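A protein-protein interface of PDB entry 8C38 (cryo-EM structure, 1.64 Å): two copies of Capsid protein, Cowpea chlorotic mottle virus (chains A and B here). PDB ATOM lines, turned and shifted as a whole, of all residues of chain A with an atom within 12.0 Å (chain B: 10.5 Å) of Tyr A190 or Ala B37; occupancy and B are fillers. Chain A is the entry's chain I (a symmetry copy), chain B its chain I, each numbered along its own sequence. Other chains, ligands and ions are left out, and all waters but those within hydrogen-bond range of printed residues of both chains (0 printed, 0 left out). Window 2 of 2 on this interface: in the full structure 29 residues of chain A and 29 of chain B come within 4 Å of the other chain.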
ATOM      1  N   PHE A 182     -15.974  33.110 -41.436  1.00  0.00           N
ATOM      2  CA  PHE A 182     -15.304  32.146 -40.568  1.00  0.00           C
ATOM      3  C   PHE A 182     -13.843  32.508 -40.341  1.00  0.00           C
ATOM      4  O   PHE A 182     -13.267  32.137 -39.312  1.00  0.00           O
ATOM      5  CB  PHE A 182     -15.413  30.745 -41.170  1.00  0.00           C
ATOM      6  CG  PHE A 182     -14.965  29.649 -40.243  1.00  0.00           C
ATOM      7  CD1 PHE A 182     -15.290  29.679 -38.896  1.00  0.00           C
ATOM      8  CD2 PHE A 182     -14.222  28.586 -40.719  1.00  0.00           C
ATOM      9  CE1 PHE A 182     -14.881  28.672 -38.046  1.00  0.00           C
ATOM     10  CE2 PHE A 182     -13.813  27.574 -39.869  1.00  0.00           C
ATOM     11  CZ  PHE A 182     -14.143  27.621 -38.534  1.00  0.00           C
ATOM     12  N   SER A 185     -11.349  35.297 -37.425  1.00  0.00           N
ATOM     13  CA  SER A 185     -10.715  35.012 -36.149  1.00  0.00           C
ATOM     14  C   SER A 185      -9.798  33.807 -36.303  1.00  0.00           C
ATOM     15  O   SER A 185      -9.926  33.024 -37.245  1.00  0.00           O
ATOM     16  CB  SER A 185     -11.756  34.749 -35.055  1.00  0.00           C
ATOM     17  OG  SER A 185     -12.503  33.584 -35.345  1.00  0.00           O
ATOM     18  N   PHE A 186      -8.871  33.673 -35.359  1.00  0.00           N
ATOM     19  CA  PHE A 186      -8.012  32.501 -35.299  1.00  0.00           C
ATOM     20  C   PHE A 186      -8.797  31.295 -34.793  1.00  0.00           C
ATOM     21  O   PHE A 186      -9.830  31.427 -34.137  1.00  0.00           O
ATOM     22  CB  PHE A 186      -6.823  32.753 -34.372  1.00  0.00           C
ATOM     23  CG  PHE A 186      -5.827  33.737 -34.917  1.00  0.00           C
ATOM     24  CD1 PHE A 186      -4.781  33.308 -35.714  1.00  0.00           C
ATOM     25  CD2 PHE A 186      -5.941  35.083 -34.633  1.00  0.00           C
ATOM     26  CE1 PHE A 186      -3.859  34.209 -36.215  1.00  0.00           C
ATOM     27  CE2 PHE A 186      -5.023  35.986 -35.131  1.00  0.00           C
ATOM     28  CZ  PHE A 186      -3.985  35.546 -35.925  1.00  0.00           C
ATOM     29  N   THR A 187      -8.282  30.111 -35.096  1.00  0.00           N
ATOM     30  CA  THR A 187      -8.796  28.902 -34.473  1.00  0.00           C
ATOM     31  C   THR A 187      -8.511  28.968 -32.977  1.00  0.00           C
ATOM     32  O   THR A 187      -7.393  29.320 -32.585  1.00  0.00           O
ATOM     33  CB  THR A 187      -8.134  27.662 -35.072  1.00  0.00           C
ATOM     34  OG1 THR A 187      -8.309  27.660 -36.492  1.00  0.00           O
ATOM     35  CG2 THR A 187      -8.722  26.389 -34.472  1.00  0.00           C
ATOM     36  N   PRO A 188      -9.477  28.659 -32.115  1.00  0.00           N
ATOM     37  CA  PRO A 188      -9.165  28.622 -30.684  1.00  0.00           C
ATOM     38  C   PRO A 188      -8.025  27.653 -30.410  1.00  0.00           C
ATOM     39  O   PRO A 188      -7.989  26.541 -30.937  1.00  0.00           O
ATOM     40  CB  PRO A 188     -10.478  28.155 -30.046  1.00  0.00           C
ATOM     41  CG  PRO A 188     -11.528  28.580 -31.013  1.00  0.00           C
ATOM     42  CD  PRO A 188     -10.908  28.414 -32.372  1.00  0.00           C
ATOM     43  N   VAL A 189      -7.079  28.088 -29.572  1.00  0.00           N
ATOM     44  CA  VAL A 189      -5.923  27.252 -29.273  1.00  0.00           C
ATOM     45  C   VAL A 189      -6.276  26.082 -28.375  1.00  0.00           C
ATOM     46  O   VAL A 189      -5.445  25.190 -28.180  1.00  0.00           O
ATOM     47  CB  VAL A 189      -4.785  28.065 -28.622  1.00  0.00           C
ATOM     48  CG1 VAL A 189      -4.344  29.194 -29.552  1.00  0.00           C
ATOM     49  CG2 VAL A 189      -5.204  28.603 -27.264  1.00  0.00           C
ATOM     50  N   TYR A 190      -7.480  26.063 -27.821  1.00  0.00           N
ATOM     51  CA  TYR A 190      -7.943  24.924 -27.045  1.00  0.00           C
ATOM     52  C   TYR A 190      -9.373  24.580 -27.438  1.00  0.00           C
ATOM     53  O   TYR A 190     -10.220  25.462 -27.556  1.00  0.00           O
ATOM     54  CB  TYR A 190      -7.863  25.220 -25.550  1.00  0.00           C
ATOM     55  CG  TYR A 190      -8.014  23.990 -24.688  1.00  0.00           C
ATOM     56  CD1 TYR A 190      -6.915  23.209 -24.360  1.00  0.00           C
ATOM     57  CD2 TYR A 190      -9.257  23.604 -24.209  1.00  0.00           C
ATOM     58  CE1 TYR A 190      -7.047  22.083 -23.572  1.00  0.00           C
ATOM     59  CE2 TYR A 190      -9.401  22.481 -23.419  1.00  0.00           C
ATOM     60  CZ  TYR A 190      -8.293  21.723 -23.106  1.00  0.00           C
ATOM     61  OH  TYR A 190      -8.430  20.602 -22.320  1.00  0.00           O
ATOM     62  OXT TYR A 190      -9.710  23.414 -27.639  1.00  0.00           O
ATOM     63  N   VAL B  33     -14.122  26.704 -10.805  1.00  0.00           N
ATOM     64  CA  VAL B  33     -13.495  26.639 -12.122  1.00  0.00           C
ATOM     65  C   VAL B  33     -14.333  25.703 -12.987  1.00  0.00           C
ATOM     66  O   VAL B  33     -14.323  24.487 -12.789  1.00  0.00           O
ATOM     67  CB  VAL B  33     -12.042  26.161 -12.028  1.00  0.00           C
ATOM     68  CG1 VAL B  33     -11.456  25.938 -13.419  1.00  0.00           C
ATOM     69  CG2 VAL B  33     -11.207  27.165 -11.239  1.00  0.00           C
ATOM     70  N   GLU B  34     -15.046  26.269 -13.955  1.00  0.00           N
ATOM     71  CA  GLU B  34     -15.896  25.476 -14.835  1.00  0.00           C
ATOM     72  C   GLU B  34     -15.046  24.787 -15.896  1.00  0.00           C
ATOM     73  O   GLU B  34     -14.390  25.473 -16.687  1.00  0.00           O
ATOM     74  CB  GLU B  34     -16.938  26.364 -15.506  1.00  0.00           C
ATOM     75  CG  GLU B  34     -17.812  27.137 -14.535  1.00  0.00           C
ATOM     76  CD  GLU B  34     -18.811  26.249 -13.820  1.00  0.00           C
ATOM     77  OE1 GLU B  34     -19.038  25.116 -14.288  1.00  0.00           O
ATOM     78  OE2 GLU B  34     -19.365  26.681 -12.789  1.00  0.00           O
ATOM     79  N   PRO B  35     -15.027  23.456 -15.958  1.00  0.00           N
ATOM     80  CA  PRO B  35     -14.283  22.792 -17.033  1.00  0.00           C
ATOM     81  C   PRO B  35     -14.869  23.141 -18.391  1.00  0.00           C
ATOM     82  O   PRO B  35     -16.071  23.369 -18.535  1.00  0.00           O
ATOM     83  CB  PRO B  35     -14.441  21.300 -16.719  1.00  0.00           C
ATOM     84  CG  PRO B  35     -14.834  21.244 -15.273  1.00  0.00           C
ATOM     85  CD  PRO B  35     -15.630  22.484 -15.029  1.00  0.00           C
ATOM     86  N   ILE B  36     -13.998  23.201 -19.391  1.00  0.00           N
ATOM     87  CA  ILE B  36     -14.420  23.429 -20.765  1.00  0.00           C
ATOM     88  C   ILE B  36     -13.837  22.324 -21.629  1.00  0.00           C
ATOM     89  O   ILE B  36     -12.790  21.751 -21.316  1.00  0.00           O
ATOM     90  CB  ILE B  36     -13.993  24.819 -21.286  1.00  0.00           C
ATOM     91  CG1 ILE B  36     -12.481  25.009 -21.160  1.00  0.00           C
ATOM     92  CG2 ILE B  36     -14.733  25.919 -20.534  1.00  0.00           C
ATOM     93  CD1 ILE B  36     -11.955  26.152 -22.010  1.00  0.00           C
ATOM     94  N   ALA B  37     -14.526  22.023 -22.721  1.00  0.00           N
ATOM     95  CA  ALA B  37     -14.120  20.949 -23.611  1.00  0.00           C
ATOM     96  C   ALA B  37     -13.119  21.457 -24.637  1.00  0.00           C
ATOM     97  O   ALA B  37     -12.945  22.660 -24.830  1.00  0.00           O
ATOM     98  CB  ALA B  37     -15.331  20.352 -24.327  1.00  0.00           C
ATOM     99  N   SER B  38     -12.459  20.511 -25.298  1.00  0.00           N
ATOM    100  CA  SER B  38     -11.647  20.847 -26.455  1.00  0.00           C
ATOM    101  C   SER B  38     -12.493  21.634 -27.441  1.00  0.00           C
ATOM    102  O   SER B  38     -13.644  21.282 -27.703  1.00  0.00           O
ATOM    103  CB  SER B  38     -11.114  19.569 -27.105  1.00  0.00           C
ATOM    104  OG  SER B  38     -10.409  19.859 -28.296  1.00  0.00           O
ATOM    105  N   GLY B  39     -11.929  22.722 -27.959  1.00  0.00           N
ATOM    106  CA  GLY B  39     -12.621  23.556 -28.912  1.00  0.00           C
ATOM    107  C   GLY B  39     -13.421  24.690 -28.309  1.00  0.00           C
ATOM    108  O   GLY B  39     -13.844  25.583 -29.048  1.00  0.00           O
ATOM    109  N   GLN B  40     -13.628  24.693 -26.992  1.00  0.00           N
ATOM    110  CA  GLN B  40     -14.424  25.725 -26.338  1.00  0.00           C
ATOM    111  C   GLN B  40     -13.640  26.997 -26.044  1.00  0.00           C
ATOM    112  O   GLN B  40     -14.237  27.970 -25.577  1.00  0.00           O
ATOM    113  CB  GLN B  40     -15.001  25.196 -25.026  1.00  0.00           C
ATOM    114  CG  GLN B  40     -16.350  24.538 -25.152  1.00  0.00           C
ATOM    115  CD  GLN B  40     -16.997  24.317 -23.799  1.00  0.00           C
ATOM    116  OE1 GLN B  40     -16.697  23.347 -23.115  1.00  0.00           O
ATOM    117  NE2 GLN B  40     -17.877  25.226 -23.407  1.00  0.00           N
ATOM    118  N   GLY B  41     -12.332  27.013 -26.286  1.00  0.00           N
ATOM    119  CA  GLY B  41     -11.561  28.211 -26.010  1.00  0.00           C
ATOM    120  C   GLY B  41     -12.098  29.410 -26.769  1.00  0.00           C
ATOM    121  O   GLY B  41     -12.660  29.287 -27.858  1.00  0.00           O
ATOM    122  N   LYS B  42     -11.939  30.586 -26.170  1.00  0.00           N
ATOM    123  CA  LYS B  42     -12.333  31.817 -26.837  1.00  0.00           C
ATOM    124  C   LYS B  42     -11.467  32.032 -28.071  1.00  0.00           C
ATOM    125  O   LYS B  42     -10.243  31.897 -28.012  1.00  0.00           O
ATOM    126  CB  LYS B  42     -12.202  32.998 -25.875  1.00  0.00           C
ATOM    127  CG  LYS B  42     -12.348  34.360 -26.529  1.00  0.00           C
ATOM    128  CD  LYS B  42     -12.588  35.446 -25.489  1.00  0.00           C
ATOM    129  CE  LYS B  42     -14.051  35.518 -25.078  1.00  0.00           C
ATOM    130  NZ  LYS B  42     -14.942  35.911 -26.204  1.00  0.00           N
ATOM    131  N   ALA B  43     -12.102  32.362 -29.192  1.00  0.00           N
ATOM    132  CA  ALA B  43     -11.368  32.582 -30.429  1.00  0.00           C
ATOM    133  C   ALA B  43     -10.819  33.999 -30.471  1.00  0.00           C
ATOM    134  O   ALA B  43     -11.509  34.957 -30.113  1.00  0.00           O
ATOM    135  CB  ALA B  43     -12.266  32.333 -31.641  1.00  0.00           C
ATOM    136  N   ILE B  44      -9.572  34.126 -30.908  1.00  0.00           N
ATOM    137  CA  ILE B  44      -8.936  35.432 -31.027  1.00  0.00           C
ATOM    138  C   ILE B  44      -9.463  36.108 -32.285  1.00  0.00           C
ATOM    139  O   ILE B  44      -9.275  35.608 -33.398  1.00  0.00           O
ATOM    140  CB  ILE B  44      -7.407  35.303 -31.062  1.00  0.00           C
ATOM    141  CG1 ILE B  44      -6.899  34.728 -29.737  1.00  0.00           C
ATOM    142  CG2 ILE B  44      -6.758  36.656 -31.338  1.00  0.00           C
ATOM    143  CD1 ILE B  44      -5.467  34.240 -29.791  1.00  0.00           C
ATOM    144  N   LEU B  92      -0.274  32.502 -35.869  1.00  0.00           N
ATOM    145  CA  LEU B  92      -0.540  31.365 -35.001  1.00  0.00           C
ATOM    146  C   LEU B  92      -0.104  30.092 -35.704  1.00  0.00           C
ATOM    147  O   LEU B  92      -0.325  29.927 -36.904  1.00  0.00           O
ATOM    148  CB  LEU B  92      -2.025  31.274 -34.630  1.00  0.00           C
ATOM    149  CG  LEU B  92      -2.452  30.057 -33.803  1.00  0.00           C
ATOM    150  CD1 LEU B  92      -1.814  30.060 -32.420  1.00  0.00           C
ATOM    151  CD2 LEU B  92      -3.965  30.019 -33.688  1.00  0.00           C
ATOM    152  N   LEU B  93       0.523  29.201 -34.942  1.00  0.00           N
ATOM    153  CA  LEU B  93       1.012  27.924 -35.434  1.00  0.00           C
ATOM    154  C   LEU B  93       0.473  26.821 -34.537  1.00  0.00           C
ATOM    155  O   LEU B  93       0.579  26.912 -33.310  1.00  0.00           O
ATOM    156  CB  LEU B  93       2.547  27.900 -35.446  1.00  0.00           C
ATOM    157  CG  LEU B  93       3.246  26.562 -35.674  1.00  0.00           C
ATOM    158  CD1 LEU B  93       3.242  26.234 -37.137  1.00  0.00           C
ATOM    159  CD2 LEU B  93       4.669  26.620 -35.140  1.00  0.00           C
ATOM    160  N   TRP B  94      -0.110  25.789 -35.136  1.00  0.00           N
ATOM    161  CA  TRP B  94      -0.513  24.626 -34.364  1.00  0.00           C
ATOM    162  C   TRP B  94      -0.367  23.391 -35.238  1.00  0.00           C
ATOM    163  O   TRP B  94      -0.160  23.478 -36.449  1.00  0.00           O
ATOM    164  CB  TRP B  94      -1.932  24.776 -33.797  1.00  0.00           C
ATOM    165  CG  TRP B  94      -3.034  24.987 -34.791  1.00  0.00           C
ATOM    166  CD1 TRP B  94      -3.378  26.156 -35.406  1.00  0.00           C
ATOM    167  CD2 TRP B  94      -3.969  24.002 -35.248  1.00  0.00           C
ATOM    168  NE1 TRP B  94      -4.460  25.954 -36.232  1.00  0.00           N
ATOM    169  CE2 TRP B  94      -4.840  24.640 -36.152  1.00  0.00           C
ATOM    170  CE3 TRP B  94      -4.145  22.641 -34.988  1.00  0.00           C
ATOM    171  CZ2 TRP B  94      -5.876  23.962 -36.796  1.00  0.00           C
ATOM    172  CZ3 TRP B  94      -5.170  21.968 -35.631  1.00  0.00           C
ATOM    173  CH2 TRP B  94      -6.022  22.631 -36.523  1.00  0.00           C
ATOM    174  N   LEU B  95      -0.446  22.231 -34.599  1.00  0.00           N
ATOM    175  CA  LEU B  95      -0.077  20.971 -35.217  1.00  0.00           C
ATOM    176  C   LEU B  95      -1.276  20.043 -35.308  1.00  0.00           C
ATOM    177  O   LEU B  95      -2.087  19.966 -34.382  1.00  0.00           O
ATOM    178  CB  LEU B  95       1.033  20.285 -34.427  1.00  0.00           C
ATOM    179  CG  LEU B  95       2.303  21.127 -34.325  1.00  0.00           C
ATOM    180  CD1 LEU B  95       3.302  20.488 -33.379  1.00  0.00           C
ATOM    181  CD2 LEU B  95       2.902  21.323 -35.708  1.00  0.00           C
ATOM    182  N   LYS B 131       2.804  19.721 -24.114  1.00  0.00           N
ATOM    183  CA  LYS B 131       2.152  20.757 -23.331  1.00  0.00           C
ATOM    184  C   LYS B 131       0.637  20.611 -23.395  1.00  0.00           C
ATOM    185  O   LYS B 131       0.085  19.952 -24.276  1.00  0.00           O
ATOM    186  CB  LYS B 131       2.556  22.144 -23.833  1.00  0.00           C
ATOM    187  CG  LYS B 131       4.051  22.354 -23.932  1.00  0.00           C
ATOM    188  CD  LYS B 131       4.747  22.096 -22.609  1.00  0.00           C
ATOM    189  CE  LYS B 131       6.137  22.713 -22.581  1.00  0.00           C
ATOM    190  NZ  LYS B 131       6.607  22.961 -21.191  1.00  0.00           N
ATOM    191  N   ASP B 132      -0.036  21.251 -22.436  1.00  0.00           N
ATOM    192  CA  ASP B 132      -1.493  21.218 -22.412  1.00  0.00           C
ATOM    193  C   ASP B 132      -2.076  21.912 -23.636  1.00  0.00           C
ATOM    194  O   ASP B 132      -3.066  21.446 -24.211  1.00  0.00           O
ATOM    195  CB  ASP B 132      -2.006  21.866 -21.127  1.00  0.00           C
ATOM    196  CG  ASP B 132      -1.508  21.157 -19.880  1.00  0.00           C
ATOM    197  OD1 ASP B 132      -1.447  19.911 -19.890  1.00  0.00           O
ATOM    198  OD2 ASP B 132      -1.176  21.844 -18.891  1.00  0.00           O
ATOM    199  N   VAL B 133      -1.476  23.025 -24.051  1.00  0.00           N
ATOM    200  CA  VAL B 133      -1.888  23.759 -25.242  1.00  0.00           C
ATOM    201  C   VAL B 133      -0.790  23.591 -26.284  1.00  0.00           C
ATOM    202  O   VAL B 133       0.340  24.050 -26.084  1.00  0.00           O
ATOM    203  CB  VAL B 133      -2.140  25.241 -24.939  1.00  0.00           C
ATOM    204  CG1 VAL B 133      -2.473  25.987 -26.214  1.00  0.00           C
ATOM    205  CG2 VAL B 133      -3.256  25.389 -23.916  1.00  0.00           C
ATOM    206  N   VAL B 134      -1.122  22.936 -27.393  1.00  0.00           N
ATOM    207  CA  VAL B 134      -0.166  22.667 -28.468  1.00  0.00           C
ATOM    208  C   VAL B 134      -0.381  23.748 -29.522  1.00  0.00           C
ATOM    209  O   VAL B 134      -1.160  23.591 -30.460  1.00  0.00           O
ATOM    210  CB  VAL B 134      -0.334  21.263 -29.039  1.00  0.00           C
ATOM    211  CG1 VAL B 134       0.768  20.972 -30.055  1.00  0.00           C
ATOM    212  CG2 VAL B 134      -0.325  20.236 -27.914  1.00  0.00           C
ATOM    213  N   ALA B 135       0.328  24.858 -29.369  1.00  0.00           N
ATOM    214  CA  ALA B 135       0.168  25.974 -30.285  1.00  0.00           C
ATOM    215  C   ALA B 135       1.204  27.027 -29.941  1.00  0.00           C
ATOM    216  O   ALA B 135       1.588  27.174 -28.779  1.00  0.00           O
ATOM    217  CB  ALA B 135      -1.241  26.572 -30.211  1.00  0.00           C
ATOM    218  N   ALA B 136       1.649  27.747 -30.963  1.00  0.00           N
ATOM    219  CA  ALA B 136       2.616  28.823 -30.801  1.00  0.00           C
ATOM    220  C   ALA B 136       2.017  30.077 -31.408  1.00  0.00           C
ATOM    221  O   ALA B 136       1.642  30.077 -32.583  1.00  0.00           O
ATOM    222  CB  ALA B 136       3.947  28.476 -31.470  1.00  0.00           C
ATOM    223  N   GLU B 174      -1.763  30.077 -39.337  1.00  0.00           N
ATOM    224  CA  GLU B 174      -2.826  31.069 -39.427  1.00  0.00           C
ATOM    225  C   GLU B 174      -2.187  32.450 -39.371  1.00  0.00           C
ATOM    226  O   GLU B 174      -1.583  32.812 -38.357  1.00  0.00           O
ATOM    227  CB  GLU B 174      -3.844  30.874 -38.304  1.00  0.00           C
ATOM    228  CG  GLU B 174      -4.340  29.434 -38.216  1.00  0.00           C
ATOM    229  CD  GLU B 174      -5.613  29.281 -37.406  1.00  0.00           C
ATOM    230  OE1 GLU B 174      -6.056  30.263 -36.780  1.00  0.00           O
ATOM    231  OE2 GLU B 174      -6.166  28.162 -37.396  1.00  0.00           O
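The backbone NH (N) of Leu B92 is in hydrogen-bond range of the backbone carbonyl oxygen (O) of Glu B174 (2.8 Å). NE1 of Trp B94 lies within hydrogen-bond range of OE2 of Glu B174 (3.0 Å). OE1 of Gln B40 lies within hydrogen-bond range of N of Ala B37.
Among the printed residues, pairs that only touch across the chains: Ser A185 with Ile B44 (3.1 Å), Pro A188 with Gly B41 (3.3 Å), Tyr A190 with Ser B38 (3.3 Å), Phe A186 with Glu B174 (3.3 Å), Tyr A190 with Gln B40 (3.5 Å), Phe A186 with Leu B92 (3.6 Å), Phe A186 with Ala B43 (3.6 Å), Val A189 with Val B133 (3.7 Å), Thr A187 with Leu B92 (3.7 Å), Tyr A190 with Ala B37 (3.8 Å), Pro A188 with Ala B43 (3.9 Å), Ser A185 with Ala B43 (3.9 Å) and Val A189 with Leu B92 (3.9 Å).
N of Gly B39 sits close to O of Tyr A190 (3.3 Å). The backbone carbonyl oxygen (O) of Ile B44 is in hydrogen-bond range of the backbone NH (N) of Phe A186. The backbone NH of Gly B41 is in hydrogen-bond range of the chain-end carboxylate of Tyr A190 (2.9 Å). The side-chain carboxylate (OE1) of Glu B174 lies within hydrogen-bond range of the backbone NH (N) of Thr A187 (2.8 Å).
Of the 7 printed residues of chain A, 6 touch a printed residue of chain B. Printed residues of chain A that touch a printed residue of chain B: Ser A185, Phe A186, Thr A187, Pro A188, Val A189 and Tyr A190. Hydrophobic or aromatic side chains of chain A that line the printed part of chain B: Phe A186, Pro A188, Val A189 and Tyr A190. Of the 23 printed residues of chain B, 10 touch a printed residue of chain A. Hydrophobic or aromatic side chains of chain B within 4 Å of the printed part of chain A: Ala B43, Ile B44, Leu B92 and Val B133. Among the printed residues, 17 pairs touch across the chains.
Of chain B, only Ala B37, Ser B38, Gly B39, Gln B40 and Gly B41 come within 4 Å of Tyr A190. Ala B37 touches just one residue of chain A: Tyr A190 (3.8 Å). Pro A188 touches just these residues of chain B: Gly B41 and Ala B43. Pro B35 touches none of the printed residues of chain A. Ser B38 touches one residue of chain A. Gly B39 touches just one residue of chain A: Tyr A190 (2.3 Å). Gln B40 touches one residue of chain A. Gly B41 touches just these residues of chain A: Pro A188 (3.3 Å) and Tyr A190 (2.9 Å). No residue of chain A comes within 4 Å of Asp B132. Printed residues of chain A within 4 Å of Glu B174: Phe A186 (3.3 Å) and Thr A187 (2.4 Å). Printed residues of chain B within 4 Å of Thr A187: Leu B92 (3.7 Å) and Glu B174 (2.4 Å). Printed residues of chain A within 4 Å of Ala B43: Ser A185, Phe A186 and Pro A188. Printed residues of chain A within 4 Å of Leu B92: Phe A186 (3.6 Å), Thr A187 (3.7 Å) and Val A189 (3.9 Å). Phe A182 touches none of the printed residues of chain B. The nearest printed residue of chain B that does not touch Tyr A190 is Ile B36 (4.1 Å). The nearest residue of chain A that does not touch Ala B37 is Pro A188 (8.0 Å). The nearest printed residue of chain A that does not touch Ala B43 is Thr A187 (5.2 Å).
No position is printed for both chains. Of the 17 pairs that touch across the chains among the printed residues, none has its exchanged pair printed and touching as well.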
